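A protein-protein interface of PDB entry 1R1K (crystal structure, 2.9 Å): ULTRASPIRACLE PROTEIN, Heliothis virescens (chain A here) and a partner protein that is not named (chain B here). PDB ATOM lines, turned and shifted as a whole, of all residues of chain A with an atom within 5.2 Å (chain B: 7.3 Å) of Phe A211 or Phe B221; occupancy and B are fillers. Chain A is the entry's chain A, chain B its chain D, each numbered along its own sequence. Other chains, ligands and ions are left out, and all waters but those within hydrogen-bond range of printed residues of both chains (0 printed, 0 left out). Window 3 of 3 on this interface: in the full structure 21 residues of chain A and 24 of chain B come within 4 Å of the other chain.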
ATOM      1  N   PHE A 193     -10.310  -7.994 -35.467  1.00  0.00           N
ATOM      2  CA  PHE A 193     -11.464  -7.583 -34.656  1.00  0.00           C
ATOM      3  C   PHE A 193     -12.547  -8.654 -34.676  1.00  0.00           C
ATOM      4  O   PHE A 193     -13.280  -8.855 -33.688  1.00  0.00           O
ATOM      5  CB  PHE A 193     -12.061  -6.265 -35.169  1.00  0.00           C
ATOM      6  CG  PHE A 193     -11.377  -5.037 -34.642  1.00  0.00           C
ATOM      7  CD1 PHE A 193     -11.252  -4.828 -33.275  1.00  0.00           C
ATOM      8  CD2 PHE A 193     -10.860  -4.084 -35.511  1.00  0.00           C
ATOM      9  CE1 PHE A 193     -10.627  -3.696 -32.789  1.00  0.00           C
ATOM     10  CE2 PHE A 193     -10.234  -2.949 -35.016  1.00  0.00           C
ATOM     11  CZ  PHE A 193     -10.121  -2.763 -33.659  1.00  0.00           C
ATOM     12  N   LEU A 196     -11.460 -12.211 -32.931  1.00  0.00           N
ATOM     13  CA  LEU A 196     -11.592 -12.024 -31.483  1.00  0.00           C
ATOM     14  C   LEU A 196     -13.025 -12.073 -30.955  1.00  0.00           C
ATOM     15  O   LEU A 196     -13.298 -12.725 -29.938  1.00  0.00           O
ATOM     16  CB  LEU A 196     -10.963 -10.692 -31.058  1.00  0.00           C
ATOM     17  CG  LEU A 196     -11.238 -10.268 -29.602  1.00  0.00           C
ATOM     18  CD1 LEU A 196     -10.655 -11.265 -28.596  1.00  0.00           C
ATOM     19  CD2 LEU A 196     -10.655  -8.885 -29.389  1.00  0.00           C
ATOM     20  N   ASP A 197     -13.915 -11.360 -31.647  1.00  0.00           N
ATOM     21  CA  ASP A 197     -15.333 -11.264 -31.298  1.00  0.00           C
ATOM     22  C   ASP A 197     -16.011 -12.615 -31.282  1.00  0.00           C
ATOM     23  O   ASP A 197     -16.826 -12.885 -30.417  1.00  0.00           O
ATOM     24  CB  ASP A 197     -16.055 -10.340 -32.291  1.00  0.00           C
ATOM     25  CG  ASP A 197     -17.482  -9.997 -31.861  1.00  0.00           C
ATOM     26  OD1 ASP A 197     -17.756  -9.845 -30.647  1.00  0.00           O
ATOM     27  OD2 ASP A 197     -18.337  -9.858 -32.758  1.00  0.00           O
ATOM     28  N   CYS A 200     -14.815 -14.774 -28.367  1.00  0.00           N
ATOM     29  CA  CYS A 200     -15.499 -14.461 -27.134  1.00  0.00           C
ATOM     30  C   CYS A 200     -16.858 -15.136 -27.215  1.00  0.00           C
ATOM     31  O   CYS A 200     -17.292 -15.782 -26.264  1.00  0.00           O
ATOM     32  CB  CYS A 200     -15.620 -12.954 -26.995  1.00  0.00           C
ATOM     33  SG  CYS A 200     -13.992 -12.224 -27.145  1.00  0.00           S
ATOM     34  N   GLY A 209     -20.083  -8.094 -22.635  1.00  0.00           N
ATOM     35  CA  GLY A 209     -19.065  -7.068 -22.788  1.00  0.00           C
ATOM     36  C   GLY A 209     -17.601  -7.439 -22.608  1.00  0.00           C
ATOM     37  O   GLY A 209     -16.803  -6.590 -22.217  1.00  0.00           O
ATOM     38  N   ARG A 210     -17.240  -8.684 -22.899  1.00  0.00           N
ATOM     39  CA  ARG A 210     -15.859  -9.107 -22.767  1.00  0.00           C
ATOM     40  C   ARG A 210     -15.034  -8.450 -23.871  1.00  0.00           C
ATOM     41  O   ARG A 210     -13.950  -7.893 -23.631  1.00  0.00           O
ATOM     42  CB  ARG A 210     -15.746 -10.622 -22.886  1.00  0.00           C
ATOM     43  CG  ARG A 210     -14.366 -11.120 -22.519  1.00  0.00           C
ATOM     44  CD  ARG A 210     -14.150 -12.583 -22.832  1.00  0.00           C
ATOM     45  NE  ARG A 210     -12.888 -13.045 -22.266  1.00  0.00           N
ATOM     46  CZ  ARG A 210     -12.606 -13.032 -20.967  1.00  0.00           C
ATOM     47  NH1 ARG A 210     -13.503 -12.590 -20.096  1.00  0.00           N
ATOM     48  NH2 ARG A 210     -11.424 -13.444 -20.542  1.00  0.00           N
ATOM     49  N   PHE A 211     -15.557  -8.531 -25.086  1.00  0.00           N
ATOM     50  CA  PHE A 211     -14.908  -7.959 -26.258  1.00  0.00           C
ATOM     51  C   PHE A 211     -14.425  -6.541 -25.974  1.00  0.00           C
ATOM     52  O   PHE A 211     -13.359  -6.135 -26.434  1.00  0.00           O
ATOM     53  CB  PHE A 211     -15.905  -7.925 -27.421  1.00  0.00           C
ATOM     54  CG  PHE A 211     -15.341  -7.374 -28.694  1.00  0.00           C
ATOM     55  CD1 PHE A 211     -14.378  -8.069 -29.395  1.00  0.00           C
ATOM     56  CD2 PHE A 211     -15.800  -6.171 -29.207  1.00  0.00           C
ATOM     57  CE1 PHE A 211     -13.883  -7.577 -30.596  1.00  0.00           C
ATOM     58  CE2 PHE A 211     -15.305  -5.678 -30.412  1.00  0.00           C
ATOM     59  CZ  PHE A 211     -14.345  -6.390 -31.103  1.00  0.00           C
ATOM     60  N   ALA A 212     -15.232  -5.791 -25.229  1.00  0.00           N
ATOM     61  CA  ALA A 212     -14.903  -4.418 -24.892  1.00  0.00           C
ATOM     62  C   ALA A 212     -13.914  -4.325 -23.744  1.00  0.00           C
ATOM     63  O   ALA A 212     -13.017  -3.490 -23.757  1.00  0.00           O
ATOM     64  CB  ALA A 212     -16.153  -3.661 -24.545  1.00  0.00           C
ATOM     65  N   ALA A 213     -14.084  -5.186 -22.747  1.00  0.00           N
ATOM     66  CA  ALA A 213     -13.195  -5.188 -21.590  1.00  0.00           C
ATOM     67  C   ALA A 213     -11.775  -5.563 -22.014  1.00  0.00           C
ATOM     68  O   ALA A 213     -10.797  -5.102 -21.407  1.00  0.00           O
ATOM     69  CB  ALA A 213     -13.704  -6.143 -20.535  1.00  0.00           C
ATOM     70  N   LEU A 214     -11.651  -6.391 -23.049  1.00  0.00           N
ATOM     71  CA  LEU A 214     -10.319  -6.759 -23.514  1.00  0.00           C
ATOM     72  C   LEU A 214      -9.729  -5.572 -24.284  1.00  0.00           C
ATOM     73  O   LEU A 214      -8.565  -5.181 -24.085  1.00  0.00           O
ATOM     74  CB  LEU A 214     -10.359  -7.983 -24.438  1.00  0.00           C
ATOM     75  CG  LEU A 214     -10.849  -9.338 -23.930  1.00  0.00           C
ATOM     76  CD1 LEU A 214     -10.708 -10.366 -25.049  1.00  0.00           C
ATOM     77  CD2 LEU A 214     -10.044  -9.766 -22.736  1.00  0.00           C
ATOM     78  N   LEU A 215     -10.540  -4.996 -25.164  1.00  0.00           N
ATOM     79  CA  LEU A 215     -10.087  -3.864 -25.961  1.00  0.00           C
ATOM     80  C   LEU A 215      -9.911  -2.590 -25.145  1.00  0.00           C
ATOM     81  O   LEU A 215      -9.333  -1.622 -25.634  1.00  0.00           O
ATOM     82  CB  LEU A 215     -11.051  -3.610 -27.115  1.00  0.00           C
ATOM     83  CG  LEU A 215     -10.895  -4.646 -28.218  1.00  0.00           C
ATOM     84  CD1 LEU A 215     -11.879  -4.377 -29.351  1.00  0.00           C
ATOM     85  CD2 LEU A 215      -9.481  -4.592 -28.735  1.00  0.00           C
ATOM     86  N   ILE B 177     -18.425   7.351 -22.325  1.00  0.00           N
ATOM     87  CA  ILE B 177     -17.499   6.280 -22.017  1.00  0.00           C
ATOM     88  C   ILE B 177     -16.165   6.822 -21.486  1.00  0.00           C
ATOM     89  O   ILE B 177     -15.772   6.518 -20.354  1.00  0.00           O
ATOM     90  CB  ILE B 177     -17.286   5.416 -23.260  1.00  0.00           C
ATOM     91  CG1 ILE B 177     -18.632   4.792 -23.653  1.00  0.00           C
ATOM     92  CG2 ILE B 177     -16.205   4.386 -22.995  1.00  0.00           C
ATOM     93  CD1 ILE B 177     -18.584   3.691 -24.700  1.00  0.00           C
ATOM     94  N   TYR B 199     -22.877   2.577 -20.750  1.00  0.00           N
ATOM     95  CA  TYR B 199     -22.666   3.285 -22.001  1.00  0.00           C
ATOM     96  C   TYR B 199     -21.957   2.392 -23.012  1.00  0.00           C
ATOM     97  O   TYR B 199     -22.271   2.404 -24.208  1.00  0.00           O
ATOM     98  CB  TYR B 199     -21.855   4.542 -21.750  1.00  0.00           C
ATOM     99  CG  TYR B 199     -22.547   5.514 -20.833  1.00  0.00           C
ATOM    100  CD1 TYR B 199     -23.293   6.569 -21.340  1.00  0.00           C
ATOM    101  CD2 TYR B 199     -22.450   5.380 -19.445  1.00  0.00           C
ATOM    102  CE1 TYR B 199     -23.922   7.476 -20.486  1.00  0.00           C
ATOM    103  CE2 TYR B 199     -23.070   6.276 -18.581  1.00  0.00           C
ATOM    104  CZ  TYR B 199     -23.802   7.325 -19.103  1.00  0.00           C
ATOM    105  OH  TYR B 199     -24.381   8.242 -18.250  1.00  0.00           O
ATOM    106  N   LEU B 200     -21.004   1.605 -22.530  1.00  0.00           N
ATOM    107  CA  LEU B 200     -20.274   0.732 -23.419  1.00  0.00           C
ATOM    108  C   LEU B 200     -21.262  -0.221 -24.067  1.00  0.00           C
ATOM    109  O   LEU B 200     -21.193  -0.515 -25.272  1.00  0.00           O
ATOM    110  CB  LEU B 200     -19.218  -0.051 -22.644  1.00  0.00           C
ATOM    111  CG  LEU B 200     -17.775   0.161 -23.115  1.00  0.00           C
ATOM    112  CD1 LEU B 200     -16.947  -1.025 -22.696  1.00  0.00           C
ATOM    113  CD2 LEU B 200     -17.715   0.319 -24.625  1.00  0.00           C
ATOM    114  N   ASN B 201     -22.198  -0.682 -23.236  1.00  0.00           N
ATOM    115  CA  ASN B 201     -23.221  -1.624 -23.666  1.00  0.00           C
ATOM    116  C   ASN B 201     -24.214  -0.981 -24.644  1.00  0.00           C
ATOM    117  O   ASN B 201     -24.464  -1.527 -25.727  1.00  0.00           O
ATOM    118  CB  ASN B 201     -23.935  -2.195 -22.442  1.00  0.00           C
ATOM    119  CG  ASN B 201     -24.798  -3.384 -22.786  1.00  0.00           C
ATOM    120  OD1 ASN B 201     -24.341  -4.323 -23.444  1.00  0.00           O
ATOM    121  ND2 ASN B 201     -26.058  -3.355 -22.347  1.00  0.00           N
ATOM    122  N   THR B 202     -24.774   0.168 -24.272  1.00  0.00           N
ATOM    123  CA  THR B 202     -25.684   0.886 -25.155  1.00  0.00           C
ATOM    124  C   THR B 202     -25.067   1.013 -26.564  1.00  0.00           C
ATOM    125  O   THR B 202     -25.724   0.730 -27.562  1.00  0.00           O
ATOM    126  CB  THR B 202     -25.961   2.314 -24.630  1.00  0.00           C
ATOM    127  OG1 THR B 202     -26.503   2.249 -23.307  1.00  0.00           O
ATOM    128  CG2 THR B 202     -26.939   3.033 -25.536  1.00  0.00           C
ATOM    129  N   LEU B 203     -23.803   1.436 -26.639  1.00  0.00           N
ATOM    130  CA  LEU B 203     -23.124   1.605 -27.920  1.00  0.00           C
ATOM    131  C   LEU B 203     -23.105   0.310 -28.694  1.00  0.00           C
ATOM    132  O   LEU B 203     -23.271   0.306 -29.901  1.00  0.00           O
ATOM    133  CB  LEU B 203     -21.685   2.095 -27.722  1.00  0.00           C
ATOM    134  CG  LEU B 203     -20.836   2.306 -28.990  1.00  0.00           C
ATOM    135  CD1 LEU B 203     -21.528   3.225 -29.968  1.00  0.00           C
ATOM    136  CD2 LEU B 203     -19.507   2.885 -28.597  1.00  0.00           C
ATOM    137  N   ARG B 204     -22.895  -0.794 -27.994  1.00  0.00           N
ATOM    138  CA  ARG B 204     -22.865  -2.098 -28.639  1.00  0.00           C
ATOM    139  C   ARG B 204     -24.189  -2.277 -29.366  1.00  0.00           C
ATOM    140  O   ARG B 204     -24.223  -2.469 -30.579  1.00  0.00           O
ATOM    141  CB  ARG B 204     -22.704  -3.197 -27.591  1.00  0.00           C
ATOM    142  CG  ARG B 204     -22.126  -4.498 -28.124  1.00  0.00           C
ATOM    143  CD  ARG B 204     -22.341  -5.601 -27.113  1.00  0.00           C
ATOM    144  NE  ARG B 204     -23.763  -5.929 -26.992  1.00  0.00           N
ATOM    145  CZ  ARG B 204     -24.352  -6.316 -25.865  1.00  0.00           C
ATOM    146  NH1 ARG B 204     -23.637  -6.419 -24.751  1.00  0.00           N
ATOM    147  NH2 ARG B 204     -25.650  -6.613 -25.847  1.00  0.00           N
ATOM    148  N   VAL B 205     -25.279  -2.194 -28.608  1.00  0.00           N
ATOM    149  CA  VAL B 205     -26.632  -2.340 -29.148  1.00  0.00           C
ATOM    150  C   VAL B 205     -26.924  -1.437 -30.363  1.00  0.00           C
ATOM    151  O   VAL B 205     -27.262  -1.929 -31.441  1.00  0.00           O
ATOM    152  CB  VAL B 205     -27.694  -2.049 -28.052  1.00  0.00           C
ATOM    153  CG1 VAL B 205     -29.077  -1.992 -28.671  1.00  0.00           C
ATOM    154  CG2 VAL B 205     -27.642  -3.120 -26.964  1.00  0.00           C
ATOM    155  N   ILE B 207     -25.158  -0.060 -32.448  1.00  0.00           N
ATOM    156  CA  ILE B 207     -24.372  -0.376 -33.630  1.00  0.00           C
ATOM    157  C   ILE B 207     -24.980  -1.655 -34.216  1.00  0.00           C
ATOM    158  O   ILE B 207     -25.020  -1.847 -35.443  1.00  0.00           O
ATOM    159  CB  ILE B 207     -22.893  -0.626 -33.230  1.00  0.00           C
ATOM    160  CG1 ILE B 207     -22.356   0.618 -32.524  1.00  0.00           C
ATOM    161  CG2 ILE B 207     -22.035  -1.035 -34.464  1.00  0.00           C
ATOM    162  CD1 ILE B 207     -21.134   0.347 -31.670  1.00  0.00           C
ATOM    163  N   ARG B 216     -19.105  -7.369 -39.640  1.00  0.00           N
ATOM    164  CA  ARG B 216     -18.677  -5.984 -39.539  1.00  0.00           C
ATOM    165  C   ARG B 216     -19.185  -5.271 -38.298  1.00  0.00           C
ATOM    166  O   ARG B 216     -18.631  -4.256 -37.896  1.00  0.00           O
ATOM    167  CB  ARG B 216     -19.120  -5.200 -40.776  1.00  0.00           C
ATOM    168  CG  ARG B 216     -18.643  -5.786 -42.095  1.00  0.00           C
ATOM    169  CD  ARG B 216     -17.161  -6.135 -42.056  1.00  0.00           C
ATOM    170  NE  ARG B 216     -16.937  -7.579 -41.965  1.00  0.00           N
ATOM    171  CZ  ARG B 216     -16.987  -8.417 -43.000  1.00  0.00           C
ATOM    172  NH1 ARG B 216     -17.255  -7.966 -44.222  1.00  0.00           N
ATOM    173  NH2 ARG B 216     -16.760  -9.710 -42.817  1.00  0.00           N
ATOM    174  N   CYS B 217     -20.238  -5.792 -37.685  1.00  0.00           N
ATOM    175  CA  CYS B 217     -20.780  -5.156 -36.494  1.00  0.00           C
ATOM    176  C   CYS B 217     -19.733  -4.980 -35.393  1.00  0.00           C
ATOM    177  O   CYS B 217     -19.757  -3.982 -34.680  1.00  0.00           O
ATOM    178  CB  CYS B 217     -21.989  -5.938 -35.967  1.00  0.00           C
ATOM    179  SG  CYS B 217     -23.498  -4.922 -35.889  1.00  0.00           S
ATOM    180  N   ALA B 218     -18.824  -5.936 -35.242  1.00  0.00           N
ATOM    181  CA  ALA B 218     -17.780  -5.793 -34.234  1.00  0.00           C
ATOM    182  C   ALA B 218     -16.741  -4.812 -34.787  1.00  0.00           C
ATOM    183  O   ALA B 218     -16.436  -3.805 -34.151  1.00  0.00           O
ATOM    184  CB  ALA B 218     -17.125  -7.137 -33.931  1.00  0.00           C
ATOM    185  N   VAL B 219     -16.202  -5.112 -35.968  1.00  0.00           N
ATOM    186  CA  VAL B 219     -15.226  -4.248 -36.623  1.00  0.00           C
ATOM    187  C   VAL B 219     -15.527  -2.774 -36.369  1.00  0.00           C
ATOM    188  O   VAL B 219     -14.610  -1.974 -36.210  1.00  0.00           O
ATOM    189  CB  VAL B 219     -15.221  -4.448 -38.158  1.00  0.00           C
ATOM    190  CG1 VAL B 219     -14.262  -3.451 -38.807  1.00  0.00           C
ATOM    191  CG2 VAL B 219     -14.841  -5.871 -38.501  1.00  0.00           C
ATOM    192  N   ILE B 220     -16.808  -2.415 -36.346  1.00  0.00           N
ATOM    193  CA  ILE B 220     -17.191  -1.030 -36.108  1.00  0.00           C
ATOM    194  C   ILE B 220     -17.003  -0.743 -34.622  1.00  0.00           C
ATOM    195  O   ILE B 220     -16.332   0.211 -34.247  1.00  0.00           O
ATOM    196  CB  ILE B 220     -18.679  -0.759 -36.612  1.00  0.00           C
ATOM    197  CG1 ILE B 220     -18.699  -0.763 -38.154  1.00  0.00           C
ATOM    198  CG2 ILE B 220     -19.230   0.567 -36.081  1.00  0.00           C
ATOM    199  CD1 ILE B 220     -20.070  -0.917 -38.786  1.00  0.00           C
ATOM    200  N   PHE B 221     -17.560  -1.598 -33.777  1.00  0.00           N
ATOM    201  CA  PHE B 221     -17.428  -1.426 -32.338  1.00  0.00           C
ATOM    202  C   PHE B 221     -15.959  -1.302 -31.903  1.00  0.00           C
ATOM    203  O   PHE B 221     -15.641  -0.576 -30.959  1.00  0.00           O
ATOM    204  CB  PHE B 221     -18.060  -2.600 -31.610  1.00  0.00           C
ATOM    205  CG  PHE B 221     -18.256  -2.356 -30.154  1.00  0.00           C
ATOM    206  CD1 PHE B 221     -18.634  -1.093 -29.695  1.00  0.00           C
ATOM    207  CD2 PHE B 221     -18.119  -3.384 -29.240  1.00  0.00           C
ATOM    208  CE1 PHE B 221     -18.876  -0.866 -28.332  1.00  0.00           C
ATOM    209  CE2 PHE B 221     -18.360  -3.166 -27.875  1.00  0.00           C
ATOM    210  CZ  PHE B 221     -18.741  -1.908 -27.420  1.00  0.00           C
ATOM    211  N   GLY B 222     -15.079  -2.016 -32.601  1.00  0.00           N
ATOM    212  CA  GLY B 222     -13.654  -2.002 -32.301  1.00  0.00           C
ATOM    213  C   GLY B 222     -12.960  -0.714 -32.700  1.00  0.00           C
ATOM    214  O   GLY B 222     -12.354  -0.051 -31.860  1.00  0.00           O
ATOM    215  N   LYS B 223     -13.036  -0.355 -33.977  1.00  0.00           N
ATOM    216  CA  LYS B 223     -12.420   0.889 -34.435  1.00  0.00           C
ATOM    217  C   LYS B 223     -12.805   2.040 -33.504  1.00  0.00           C
ATOM    218  O   LYS B 223     -11.989   2.907 -33.192  1.00  0.00           O
ATOM    219  CB  LYS B 223     -12.856   1.213 -35.866  1.00  0.00           C
ATOM    220  CG  LYS B 223     -12.228   0.312 -36.907  1.00  0.00           C
ATOM    221  CD  LYS B 223     -12.968   0.368 -38.247  1.00  0.00           C
ATOM    222  CE  LYS B 223     -12.816   1.713 -38.949  1.00  0.00           C
ATOM    223  NZ  LYS B 223     -13.845   1.867 -40.004  1.00  0.00           N
ATOM    224  N   ILE B 224     -14.051   2.037 -33.055  1.00  0.00           N
ATOM    225  CA  ILE B 224     -14.519   3.075 -32.175  1.00  0.00           C
ATOM    226  C   ILE B 224     -13.798   2.973 -30.835  1.00  0.00           C
ATOM    227  O   ILE B 224     -13.177   3.941 -30.383  1.00  0.00           O
ATOM    228  CB  ILE B 224     -16.059   2.989 -32.020  1.00  0.00           C
ATOM    229  CG1 ILE B 224     -16.712   3.482 -33.317  1.00  0.00           C
ATOM    230  CG2 ILE B 224     -16.548   3.798 -30.806  1.00  0.00           C
ATOM    231  CD1 ILE B 224     -18.187   3.845 -33.164  1.00  0.00           C
ATOM    232  N   LEU B 225     -13.841   1.815 -30.196  1.00  0.00           N
ATOM    233  CA  LEU B 225     -13.149   1.685 -28.920  1.00  0.00           C
ATOM    234  C   LEU B 225     -11.641   2.012 -29.056  1.00  0.00           C
ATOM    235  O   LEU B 225     -10.976   2.339 -28.074  1.00  0.00           O
ATOM    236  CB  LEU B 225     -13.361   0.270 -28.337  1.00  0.00           C
ATOM    237  CG  LEU B 225     -14.751   0.021 -27.714  1.00  0.00           C
ATOM    238  CD1 LEU B 225     -14.660  -1.035 -26.668  1.00  0.00           C
ATOM    239  CD2 LEU B 225     -15.279   1.278 -27.047  1.00  0.00           C
ATOM    240  N   GLY B 226     -11.122   1.926 -30.285  1.00  0.00           N
ATOM    241  CA  GLY B 226      -9.725   2.201 -30.581  1.00  0.00           C
ATOM    242  C   GLY B 226      -9.446   3.660 -30.409  1.00  0.00           C
ATOM    243  O   GLY B 226      -8.343   4.031 -30.061  1.00  0.00           O
ATOM    244  N   ILE B 227     -10.440   4.496 -30.671  1.00  0.00           N
ATOM    245  CA  ILE B 227     -10.290   5.929 -30.490  1.00  0.00           C
ATOM    246  C   ILE B 227      -9.801   6.201 -29.044  1.00  0.00           C
ATOM    247  O   ILE B 227      -9.066   7.168 -28.765  1.00  0.00           O
ATOM    248  CB  ILE B 227     -11.640   6.644 -30.688  1.00  0.00           C
ATOM    249  CG1 ILE B 227     -12.066   6.515 -32.166  1.00  0.00           C
ATOM    250  CG2 ILE B 227     -11.556   8.102 -30.128  1.00  0.00           C
ATOM    251  CD1 ILE B 227     -13.550   6.882 -32.438  1.00  0.00           C
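Among the printed residues, merely in contact across the chains: Asp A197 with Ala B218 (3.2 Å), Ala A212 with Leu B200 (3.3 Å), Phe A193 with Gly B222 (3.5 Å), Phe A211 with Phe B221 (3.6 Å), Ala A212 with Leu B225 (3.7 Å) and Phe A193 with Lys B223 (3.8 Å).
Of chain A, only Phe A211 comes within 4 Å of Phe B221.
Printed residues of chain A within 4 Å of Leu B225: Ala A212.
Of the printed residues of chain B, Ala A212 touches Leu B200 (3.3 Å) and Leu B225 (3.7 Å).
Printed residues of chain A within 4 Å of Leu B200: Ala A212 (3.3 Å).
Of the printed residues of chain B, Phe A193 touches Gly B222 (3.5 Å) and Lys B223 (3.8 Å).
Printed residues of chain A within 4 Å of Ala B218: Asp A197.
Arg A210 touches none of the printed residues of chain B.
Gly A209 touches none of the printed residues of chain B.
The nearest residue of chain A that does not touch Phe B221 is Ala A212 (4.03 Å).
Along chain B the printed residues that touch a printed residue of chain A span positions 200 to 225.
Hydrophobic or aromatic side chains of chain A that line the printed part of chain B: Phe A193, Phe A211 and Ala A212.
Among the printed residues, 6 pairs touch across the chains.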
